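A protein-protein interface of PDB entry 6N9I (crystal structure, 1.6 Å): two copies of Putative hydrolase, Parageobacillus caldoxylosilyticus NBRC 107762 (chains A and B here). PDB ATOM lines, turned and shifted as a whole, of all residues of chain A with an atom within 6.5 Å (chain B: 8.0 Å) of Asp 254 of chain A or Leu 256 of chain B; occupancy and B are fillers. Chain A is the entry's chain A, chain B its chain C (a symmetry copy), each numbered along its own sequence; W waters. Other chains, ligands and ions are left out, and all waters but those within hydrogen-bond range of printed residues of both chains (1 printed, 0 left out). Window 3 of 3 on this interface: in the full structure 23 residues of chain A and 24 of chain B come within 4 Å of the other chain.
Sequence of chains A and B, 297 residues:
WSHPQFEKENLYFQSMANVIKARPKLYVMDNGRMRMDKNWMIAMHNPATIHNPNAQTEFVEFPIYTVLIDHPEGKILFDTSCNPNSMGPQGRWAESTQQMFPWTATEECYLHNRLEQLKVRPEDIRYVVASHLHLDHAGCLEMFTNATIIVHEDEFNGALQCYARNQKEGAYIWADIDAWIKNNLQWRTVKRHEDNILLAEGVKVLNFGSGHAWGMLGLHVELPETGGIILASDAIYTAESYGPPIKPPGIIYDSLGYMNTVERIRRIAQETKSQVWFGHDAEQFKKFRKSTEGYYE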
ATOM      1  N   GLY A 209      37.857 -20.148  28.872  1.00  0.00           N
ATOM      2  CA  GLY A 209      37.044 -18.949  28.701  1.00  0.00           C
ATOM      3  C   GLY A 209      35.677 -19.265  28.117  1.00  0.00           C
ATOM      4  O   GLY A 209      35.152 -20.372  28.277  1.00  0.00           O
ATOM      5  N   SER A 210      35.102 -18.283  27.419  1.00  0.00           N
ATOM      6  CA  SER A 210      33.715 -18.355  26.974  1.00  0.00           C
ATOM      7  C   SER A 210      33.591 -19.211  25.710  1.00  0.00           C
ATOM      8  O   SER A 210      34.456 -19.203  24.835  1.00  0.00           O
ATOM      9  CB  SER A 210      33.140 -16.974  26.762  1.00  0.00           C
ATOM     10  OG  SER A 210      33.923 -16.225  25.849  1.00  0.00           O
ATOM     11  N   GLY A 211      32.474 -19.937  25.628  1.00  0.00           N
ATOM     12  CA  GLY A 211      32.180 -20.819  24.518  1.00  0.00           C
ATOM     13  C   GLY A 211      30.839 -21.494  24.716  1.00  0.00           C
ATOM     14  O   GLY A 211      29.795 -20.859  24.554  1.00  0.00           O
ATOM     15  N   HIS A 212      30.883 -22.779  25.084  1.00  0.00           N
ATOM     16  CA  HIS A 212      29.693 -23.542  25.435  1.00  0.00           C
ATOM     17  C   HIS A 212      28.893 -22.778  26.495  1.00  0.00           C
ATOM     18  O   HIS A 212      27.674 -22.649  26.390  1.00  0.00           O
ATOM     19  CB  HIS A 212      30.081 -24.954  25.902  1.00  0.00           C
ATOM     20  CG  HIS A 212      28.988 -25.702  26.594  1.00  0.00           C
ATOM     21  ND1 HIS A 212      27.871 -26.170  25.929  1.00  0.00           N
ATOM     22  CD2 HIS A 212      28.849 -26.087  27.883  1.00  0.00           C
ATOM     23  CE1 HIS A 212      27.088 -26.800  26.782  1.00  0.00           C
ATOM     24  NE2 HIS A 212      27.666 -26.766  27.986  1.00  0.00           N
ATOM     25  N   ALA A 213      29.606 -22.278  27.510  1.00  0.00           N
ATOM     26  CA  ALA A 213      29.027 -21.514  28.606  1.00  0.00           C
ATOM     27  C   ALA A 213      29.842 -20.229  28.810  1.00  0.00           C
ATOM     28  O   ALA A 213      30.708 -19.904  28.002  1.00  0.00           O
ATOM     29  CB  ALA A 213      28.979 -22.361  29.855  1.00  0.00           C
ATOM     30  N   ILE A 252      24.925 -23.260  23.565  1.00  0.00           N
ATOM     31  CA  ILE A 252      26.111 -22.474  23.269  1.00  0.00           C
ATOM     32  C   ILE A 252      25.860 -21.008  23.643  1.00  0.00           C
ATOM     33  O   ILE A 252      24.734 -20.513  23.555  1.00  0.00           O
ATOM     34  CB  ILE A 252      26.483 -22.628  21.783  1.00  0.00           C
ATOM     35  CG1 ILE A 252      27.939 -22.239  21.513  1.00  0.00           C
ATOM     36  CG2 ILE A 252      25.515 -21.848  20.909  1.00  0.00           C
ATOM     37  CD1 ILE A 252      28.432 -22.656  20.149  1.00  0.00           C
ATOM     38  N   TYR A 253      26.932 -20.326  24.050  1.00  0.00           N
ATOM     39  CA  TYR A 253      26.889 -18.934  24.468  1.00  0.00           C
ATOM     40  C   TYR A 253      27.695 -18.065  23.491  1.00  0.00           C
ATOM     41  O   TYR A 253      27.180 -17.092  22.937  1.00  0.00           O
ATOM     42  CB  TYR A 253      27.426 -18.797  25.895  1.00  0.00           C
ATOM     43  CG  TYR A 253      27.741 -17.381  26.300  1.00  0.00           C
ATOM     44  CD1 TYR A 253      26.739 -16.431  26.393  1.00  0.00           C
ATOM     45  CD2 TYR A 253      29.039 -16.981  26.568  1.00  0.00           C
ATOM     46  CE1 TYR A 253      27.016 -15.122  26.747  1.00  0.00           C
ATOM     47  CE2 TYR A 253      29.333 -15.676  26.926  1.00  0.00           C
ATOM     48  CZ  TYR A 253      28.316 -14.741  27.011  1.00  0.00           C
ATOM     49  OH  TYR A 253      28.587 -13.451  27.358  1.00  0.00           O
ATOM     50  N   ASP A 254      28.963 -18.437  23.295  1.00  0.00           N
ATOM     51  CA  ASP A 254      29.923 -17.676  22.503  1.00  0.00           C
ATOM     52  C   ASP A 254      30.466 -18.584  21.396  1.00  0.00           C
ATOM     53  O   ASP A 254      31.400 -19.350  21.622  1.00  0.00           O
ATOM     54  CB  ASP A 254      31.044 -17.145  23.404  1.00  0.00           C
ATOM     55  CG  ASP A 254      32.219 -16.508  22.677  1.00  0.00           C
ATOM     56  OD1 ASP A 254      32.102 -16.253  21.460  1.00  0.00           O
ATOM     57  OD2 ASP A 254      33.252 -16.265  23.346  1.00  0.00           O
ATOM     58  N   SER A 255      29.864 -18.499  20.205  1.00  0.00           N
ATOM     59  CA  SER A 255      30.159 -19.436  19.120  1.00  0.00           C
ATOM     60  C   SER A 255      31.634 -19.336  18.710  1.00  0.00           C
ATOM     61  O   SER A 255      32.280 -20.359  18.496  1.00  0.00           O
ATOM     62  CB  SER A 255      29.241 -19.230  17.937  1.00  0.00           C
ATOM     63  OG  SER A 255      29.317 -17.900  17.446  1.00  0.00           O
ATOM     64  N   LEU A 256      32.155 -18.107  18.592  1.00  0.00           N
ATOM     65  CA  LEU A 256      33.544 -17.905  18.171  1.00  0.00           C
ATOM     66  C   LEU A 256      34.483 -18.505  19.221  1.00  0.00           C
ATOM     67  O   LEU A 256      35.453 -19.200  18.882  1.00  0.00           O
ATOM     68  CB  LEU A 256      33.830 -16.414  17.981  1.00  0.00           C
ATOM     69  CG  LEU A 256      33.069 -15.727  16.847  1.00  0.00           C
ATOM     70  CD1 LEU A 256      33.583 -14.313  16.642  1.00  0.00           C
ATOM     71  CD2 LEU A 256      33.164 -16.524  15.554  1.00  0.00           C
ATOM     72  N   GLY A 257      34.193 -18.212  20.492  1.00  0.00           N
ATOM     73  CA  GLY A 257      34.981 -18.711  21.609  1.00  0.00           C
ATOM     74  C   GLY A 257      34.955 -20.227  21.663  1.00  0.00           C
ATOM     75  O   GLY A 257      35.962 -20.867  21.973  1.00  0.00           O
ATOM     76  N   TYR A 258      33.789 -20.803  21.357  1.00  0.00           N
ATOM     77  CA  TYR A 258      33.622 -22.249  21.363  1.00  0.00           C
ATOM     78  C   TYR A 258      34.573 -22.875  20.340  1.00  0.00           C
ATOM     79  O   TYR A 258      35.290 -23.829  20.649  1.00  0.00           O
ATOM     80  CB  TYR A 258      32.180 -22.661  21.053  1.00  0.00           C
ATOM     81  CG  TYR A 258      32.041 -24.144  20.824  1.00  0.00           C
ATOM     82  CD1 TYR A 258      31.851 -25.019  21.882  1.00  0.00           C
ATOM     83  CD2 TYR A 258      32.159 -24.680  19.554  1.00  0.00           C
ATOM     84  CE1 TYR A 258      31.760 -26.387  21.680  1.00  0.00           C
ATOM     85  CE2 TYR A 258      32.072 -26.045  19.336  1.00  0.00           C
ATOM     86  CZ  TYR A 258      31.870 -26.902  20.402  1.00  0.00           C
ATOM     87  OH  TYR A 258      31.783 -28.248  20.183  1.00  0.00           O
ATOM     88  N   MET A 259      34.562 -22.327  19.121  1.00  0.00           N
ATOM     89  CA  MET A 259      35.368 -22.836  18.015  1.00  0.00           C
ATOM     90  C   MET A 259      36.853 -22.675  18.357  1.00  0.00           C
ATOM     91  O   MET A 259      37.646 -23.595  18.152  1.00  0.00           O
ATOM     92  CB  MET A 259      35.063 -22.088  16.713  1.00  0.00           C
ATOM     93  CG  MET A 259      33.619 -22.211  16.258  1.00  0.00           C
ATOM     94  SD  MET A 259      33.155 -23.903  15.816  1.00  0.00           S
ATOM     95  CE  MET A 259      34.104 -24.135  14.315  1.00  0.00           C
ATOM     96  N   SER B 210      30.173  -8.514  12.713  1.00  0.00           N
ATOM     97  CA  SER B 210      29.964  -9.957  12.706  1.00  0.00           C
ATOM     98  C   SER B 210      28.769 -10.340  13.589  1.00  0.00           C
ATOM     99  O   SER B 210      28.527  -9.752  14.641  1.00  0.00           O
ATOM    100  CB  SER B 210      31.217 -10.689  13.128  1.00  0.00           C
ATOM    101  OG  SER B 210      31.668 -10.246  14.397  1.00  0.00           O
ATOM    102  N   GLY B 211      28.034 -11.353  13.134  1.00  0.00           N
ATOM    103  CA  GLY B 211      26.863 -11.863  13.824  1.00  0.00           C
ATOM    104  C   GLY B 211      26.259 -13.027  13.066  1.00  0.00           C
ATOM    105  O   GLY B 211      26.799 -14.129  13.079  1.00  0.00           O
ATOM    106  N   ILE B 252      24.169 -18.899  12.121  1.00  0.00           N
ATOM    107  CA  ILE B 252      24.852 -17.894  12.922  1.00  0.00           C
ATOM    108  C   ILE B 252      26.362 -18.158  12.876  1.00  0.00           C
ATOM    109  O   ILE B 252      26.797 -19.307  12.824  1.00  0.00           O
ATOM    110  CB  ILE B 252      24.305 -17.920  14.361  1.00  0.00           C
ATOM    111  CG1 ILE B 252      24.578 -16.613  15.109  1.00  0.00           C
ATOM    112  CG2 ILE B 252      24.842 -19.129  15.111  1.00  0.00           C
ATOM    113  CD1 ILE B 252      23.745 -16.448  16.356  1.00  0.00           C
ATOM    114  N   TYR B 253      27.144 -17.074  12.886  1.00  0.00           N
ATOM    115  CA  TYR B 253      28.603 -17.142  12.871  1.00  0.00           C
ATOM    116  C   TYR B 253      29.155 -16.724  14.237  1.00  0.00           C
ATOM    117  O   TYR B 253      29.928 -17.463  14.861  1.00  0.00           O
ATOM    118  CB  TYR B 253      29.169 -16.255  11.759  1.00  0.00           C
ATOM    119  CG  TYR B 253      30.643 -15.963  11.891  1.00  0.00           C
ATOM    120  CD1 TYR B 253      31.581 -16.974  11.764  1.00  0.00           C
ATOM    121  CD2 TYR B 253      31.100 -14.681  12.147  1.00  0.00           C
ATOM    122  CE1 TYR B 253      32.935 -16.717  11.892  1.00  0.00           C
ATOM    123  CE2 TYR B 253      32.451 -14.409  12.278  1.00  0.00           C
ATOM    124  CZ  TYR B 253      33.372 -15.432  12.148  1.00  0.00           C
ATOM    125  OH  TYR B 253      34.709 -15.181  12.271  1.00  0.00           O
ATOM    126  N   ASP B 254      28.740 -15.532  14.681  1.00  0.00           N
ATOM    127  CA  ASP B 254      29.226 -14.897  15.899  1.00  0.00           C
ATOM    128  C   ASP B 254      28.026 -14.585  16.797  1.00  0.00           C
ATOM    129  O   ASP B 254      27.374 -13.562  16.624  1.00  0.00           O
ATOM    130  CB  ASP B 254      30.024 -13.635  15.555  1.00  0.00           C
ATOM    131  CG  ASP B 254      30.432 -12.777  16.742  1.00  0.00           C
ATOM    132  OD1 ASP B 254      30.301 -13.245  17.896  1.00  0.00           O
ATOM    133  OD2 ASP B 254      30.890 -11.641  16.499  1.00  0.00           O
ATOM    134  N   SER B 255      27.752 -15.475  17.756  1.00  0.00           N
ATOM    135  CA  SER B 255      26.538 -15.395  18.566  1.00  0.00           C
ATOM    136  C   SER B 255      26.539 -14.123  19.425  1.00  0.00           C
ATOM    137  O   SER B 255      25.506 -13.471  19.571  1.00  0.00           O
ATOM    138  CB  SER B 255      26.354 -16.633  19.409  1.00  0.00           C
ATOM    139  OG  SER B 255      27.477 -16.858  20.245  1.00  0.00           O
ATOM    140  N   LEU B 256      27.693 -13.776  20.002  1.00  0.00           N
ATOM    141  CA  LEU B 256      27.780 -12.585  20.842  1.00  0.00           C
ATOM    142  C   LEU B 256      27.530 -11.341  19.983  1.00  0.00           C
ATOM    143  O   LEU B 256      26.796 -10.433  20.385  1.00  0.00           O
ATOM    144  CB  LEU B 256      29.153 -12.511  21.515  1.00  0.00           C
ATOM    145  CG  LEU B 256      29.465 -13.620  22.514  1.00  0.00           C
ATOM    146  CD1 LEU B 256      30.739 -13.297  23.279  1.00  0.00           C
ATOM    147  CD2 LEU B 256      28.306 -13.842  23.476  1.00  0.00           C
ATOM    148  N   GLY B 257      28.161 -11.313  18.805  1.00  0.00           N
ATOM    149  CA  GLY B 257      28.033 -10.208  17.870  1.00  0.00           C
ATOM    150  C   GLY B 257      26.600 -10.060  17.391  1.00  0.00           C
ATOM    151  O   GLY B 257      26.098  -8.945  17.229  1.00  0.00           O
ATOM    152  N   TYR B 258      25.944 -11.200  17.163  1.00  0.00           N
ATOM    153  CA  TYR B 258      24.557 -11.212  16.727  1.00  0.00           C
ATOM    154  C   TYR B 258      23.680 -10.519  17.776  1.00  0.00           C
ATOM    155  O   TYR B 258      22.865  -9.655  17.446  1.00  0.00           O
ATOM    156  CB  TYR B 258      24.051 -12.636  16.484  1.00  0.00           C
ATOM    157  CG  TYR B 258      22.561 -12.676  16.263  1.00  0.00           C
ATOM    158  CD1 TYR B 258      21.686 -12.783  17.330  1.00  0.00           C
ATOM    159  CD2 TYR B 258      22.027 -12.547  14.994  1.00  0.00           C
ATOM    160  CE1 TYR B 258      20.314 -12.785  17.138  1.00  0.00           C
ATOM    161  CE2 TYR B 258      20.658 -12.533  14.787  1.00  0.00           C
ATOM    162  CZ  TYR B 258      19.799 -12.662  15.861  1.00  0.00           C
ATOM    163  OH  TYR B 258      18.448 -12.648  15.662  1.00  0.00           O
ATOM    164  N   MET B 259      23.854 -10.915  19.039  1.00  0.00           N
ATOM    165  CA  MET B 259      23.052 -10.389  20.138  1.00  0.00           C
ATOM    166  C   MET B 259      23.330  -8.890  20.296  1.00  0.00           C
ATOM    167  O   MET B 259      22.406  -8.096  20.467  1.00  0.00           O
ATOM    168  CB  MET B 259      23.363 -11.114  21.451  1.00  0.00           C
ATOM    169  CG  MET B 259      23.073 -12.605  21.413  1.00  0.00           C
ATOM    170  SD  MET B 259      21.321 -12.990  21.157  1.00  0.00           S
ATOM    171  CE  MET B 259      20.612 -12.350  22.672  1.00  0.00           C
ATOM    172  N   ASN B 260      24.611  -8.512  20.224  1.00  0.00           N
ATOM    173  CA  ASN B 260      25.024  -7.114  20.337  1.00  0.00           C
ATOM    174  C   ASN B 260      24.328  -6.277  19.257  1.00  0.00           C
ATOM    175  O   ASN B 260      23.873  -5.165  19.516  1.00  0.00           O
ATOM    176  CB  ASN B 260      26.541  -6.952  20.218  1.00  0.00           C
ATOM    177  CG  ASN B 260      27.294  -7.505  21.410  1.00  0.00           C
ATOM    178  OD1 ASN B 260      28.485  -7.800  21.313  1.00  0.00           O
ATOM    179  ND2 ASN B 260      26.612  -7.656  22.532  1.00  0.00           N
ATOM    180  N   THR B 261      24.274  -6.816  18.039  1.00  0.00           N
ATOM    181  CA  THR B 261      23.732  -6.082  16.903  1.00  0.00           C
ATOM    182  C   THR B 261      22.223  -5.867  17.091  1.00  0.00           C
ATOM    183  O   THR B 261      21.725  -4.772  16.862  1.00  0.00           O
ATOM    184  CB  THR B 261      24.054  -6.785  15.582  1.00  0.00           C
ATOM    185  OG1 THR B 261      25.466  -6.699  15.387  1.00  0.00           O
ATOM    186  CG2 THR B 261      23.334  -6.168  14.403  1.00  0.00           C
ATOM    187  N   VAL B 262      21.501  -6.909  17.512  1.00  0.00           N
ATOM    188  CA  VAL B 262      20.052  -6.778  17.683  1.00  0.00           C
ATOM    189  C   VAL B 262      19.770  -5.678  18.714  1.00  0.00           C
ATOM    190  O   VAL B 262      18.897  -4.827  18.502  1.00  0.00           O
ATOM    191  CB  VAL B 262      19.374  -8.100  18.086  1.00  0.00           C
ATOM    192  CG1 VAL B 262      17.892  -7.889  18.356  1.00  0.00           C
ATOM    193  CG2 VAL B 262      19.570  -9.179  17.035  1.00  0.00           C
ATOM    194  N   GLU B 263      20.516  -5.693  19.822  1.00  0.00           N
ATOM    195  CA  GLU B 263      20.295  -4.746  20.904  1.00  0.00           C
ATOM    196  C   GLU B 263      20.658  -3.334  20.432  1.00  0.00           C
ATOM    197  O   GLU B 263      20.012  -2.361  20.816  1.00  0.00           O
ATOM    198  CB  GLU B 263      21.069  -5.161  22.158  1.00  0.00           C
ATOM    199  CG  GLU B 263      20.397  -6.290  22.916  1.00  0.00           C
ATOM    200  CD  GLU B 263      18.988  -5.968  23.393  1.00  0.00           C
ATOM    201  OE1 GLU B 263      18.806  -4.911  24.030  1.00  0.00           O
ATOM    202  OE2 GLU B 263      18.073  -6.767  23.117  1.00  0.00           O
HETATM  203  O   HOH W   1      31.035 -15.862  19.028  1.00  0.00           O
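Hydrophobic or aromatic side chains of chain A that line the printed part of chain B: Tyr 253 and Leu 256.
Along chain A the printed residues that touch a printed residue of chain B span positions 253 to 256.
Among the printed residues, 9 pairs touch across the chains.
Among the printed residues, no Asp or Glu carboxylate lies within 4 Å of a Lys or Arg side-chain nitrogen of the other chain.
Among the printed residues, pairs that only touch across the chains: Tyr 253 of chain A with Leu 256 of chain B (3.5 Å), Asp 254 of chain A with Ser 255 of chain B (3.4 Å), Asp 254 of chain A with Leu 256 of chain B (3.6 Å), Ser 255 of chain A with Asp 254 of chain B (3.4 Å), Leu 256 of chain A with Tyr 253 of chain B (3.4 Å) and Leu 256 of chain A with Asp 254 of chain B (3.5 Å).
Water W1 lies within hydrogen-bond range of the backbone NH (N) of Leu 256 of chain A (2.5 Å), the side-chain carboxylate (OD1) of Asp 254 of chain A (2.7 Å), the side-chain carboxylate (OD1) of Asp 254 of chain B (2.9 Å) and the side-chain hydroxyl (OG) of Ser 255 of chain A (3.1 Å).
The side-chain hydroxyl of Ser 255 of chain B is in hydrogen-bond range of the backbone carbonyl oxygen of Tyr 253 of chain A.
OG of Ser 255 of chain A sits at hydrogen-bond distance from O of Tyr 253 of chain B (2.7 Å).
The backbone NH (N) of Ser 255 of chain A lies within hydrogen-bond range of the side-chain hydroxyl (OG) of Ser 255 of chain B (2.9 Å).
O of Gly 211 of chain A sits at hydrogen-bond distance from N of Asp 254 of chain A.
O of His 212 of chain A sits at hydrogen-bond distance from N of Tyr 253 of chain A, 3.4 Å away.
The backbone NH of Gly 257 of chain A sits at hydrogen-bond distance from the side-chain carboxylate of Asp 254 of chain A, 3.0 Å away.
OG of Ser 210 of chain B is in hydrogen-bond range of OD2 of Asp 254 of chain B, 2.6 Å away.
N of Leu 256 of chain B sits close to OD1 of Asp 254 of chain B (3.4 Å).
The side-chain carboxylate (OD1) of Asp 254 of chain B lies within hydrogen-bond range of the backbone NH (N) of Gly 257 of chain B.
Asp 254 of chain A touches just these residues of chain B: Ser 255 (3.4 Å) and Leu 256 (3.6 Å).
Leu 256 of chain B touches just these residues of chain A: Tyr 253 and Asp 254.
No residue of chain B comes within 4 Å of Gly 211 of chain A.
Of the printed residues of chain B, Ser 255 of chain A touches Tyr 253, Asp 254 and Ser 255.
Of the printed residues of chain A, Ser 255 of chain B touches Tyr 253 (2.7 Å), Asp 254 (3.4 Å) and Ser 255 (2.9 Å).
Of the printed residues of chain A, Tyr 253 of chain B touches Ser 255 and Leu 256.
Of the printed residues of chain B, Leu 256 of chain A touches Tyr 253 and Asp 254.
Met 259 of chain B touches none of the printed residues of chain A.
Gly 211 of chain B touches none of the printed residues of chain A.
The nearest residue of chain B that does not touch Asp 254 of chain A is Asp 254 of chain B (5.0 Å).
The nearest residue of chain A that does not touch Leu 256 of chain B is Ser 210 of chain A (5.0 Å).
Tyr 253 of chain A touches Leu 256 of chain B, and with the chains exchanged Leu 256 of chain A touches Tyr 253 of chain B.
Asp 254 of chain A touches Ser 255 of chain B, and with the chains exchanged Ser 255 of chain A touches Asp 254 of chain B.
Asp 254 of chain A touches Leu 256 of chain B, and with the chains exchanged Leu 256 of chain A touches Asp 254 of chain B.
Ser 255 of chain A touches its own counterpart, Ser 255 of chain B.
10 positions are printed for both chains.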
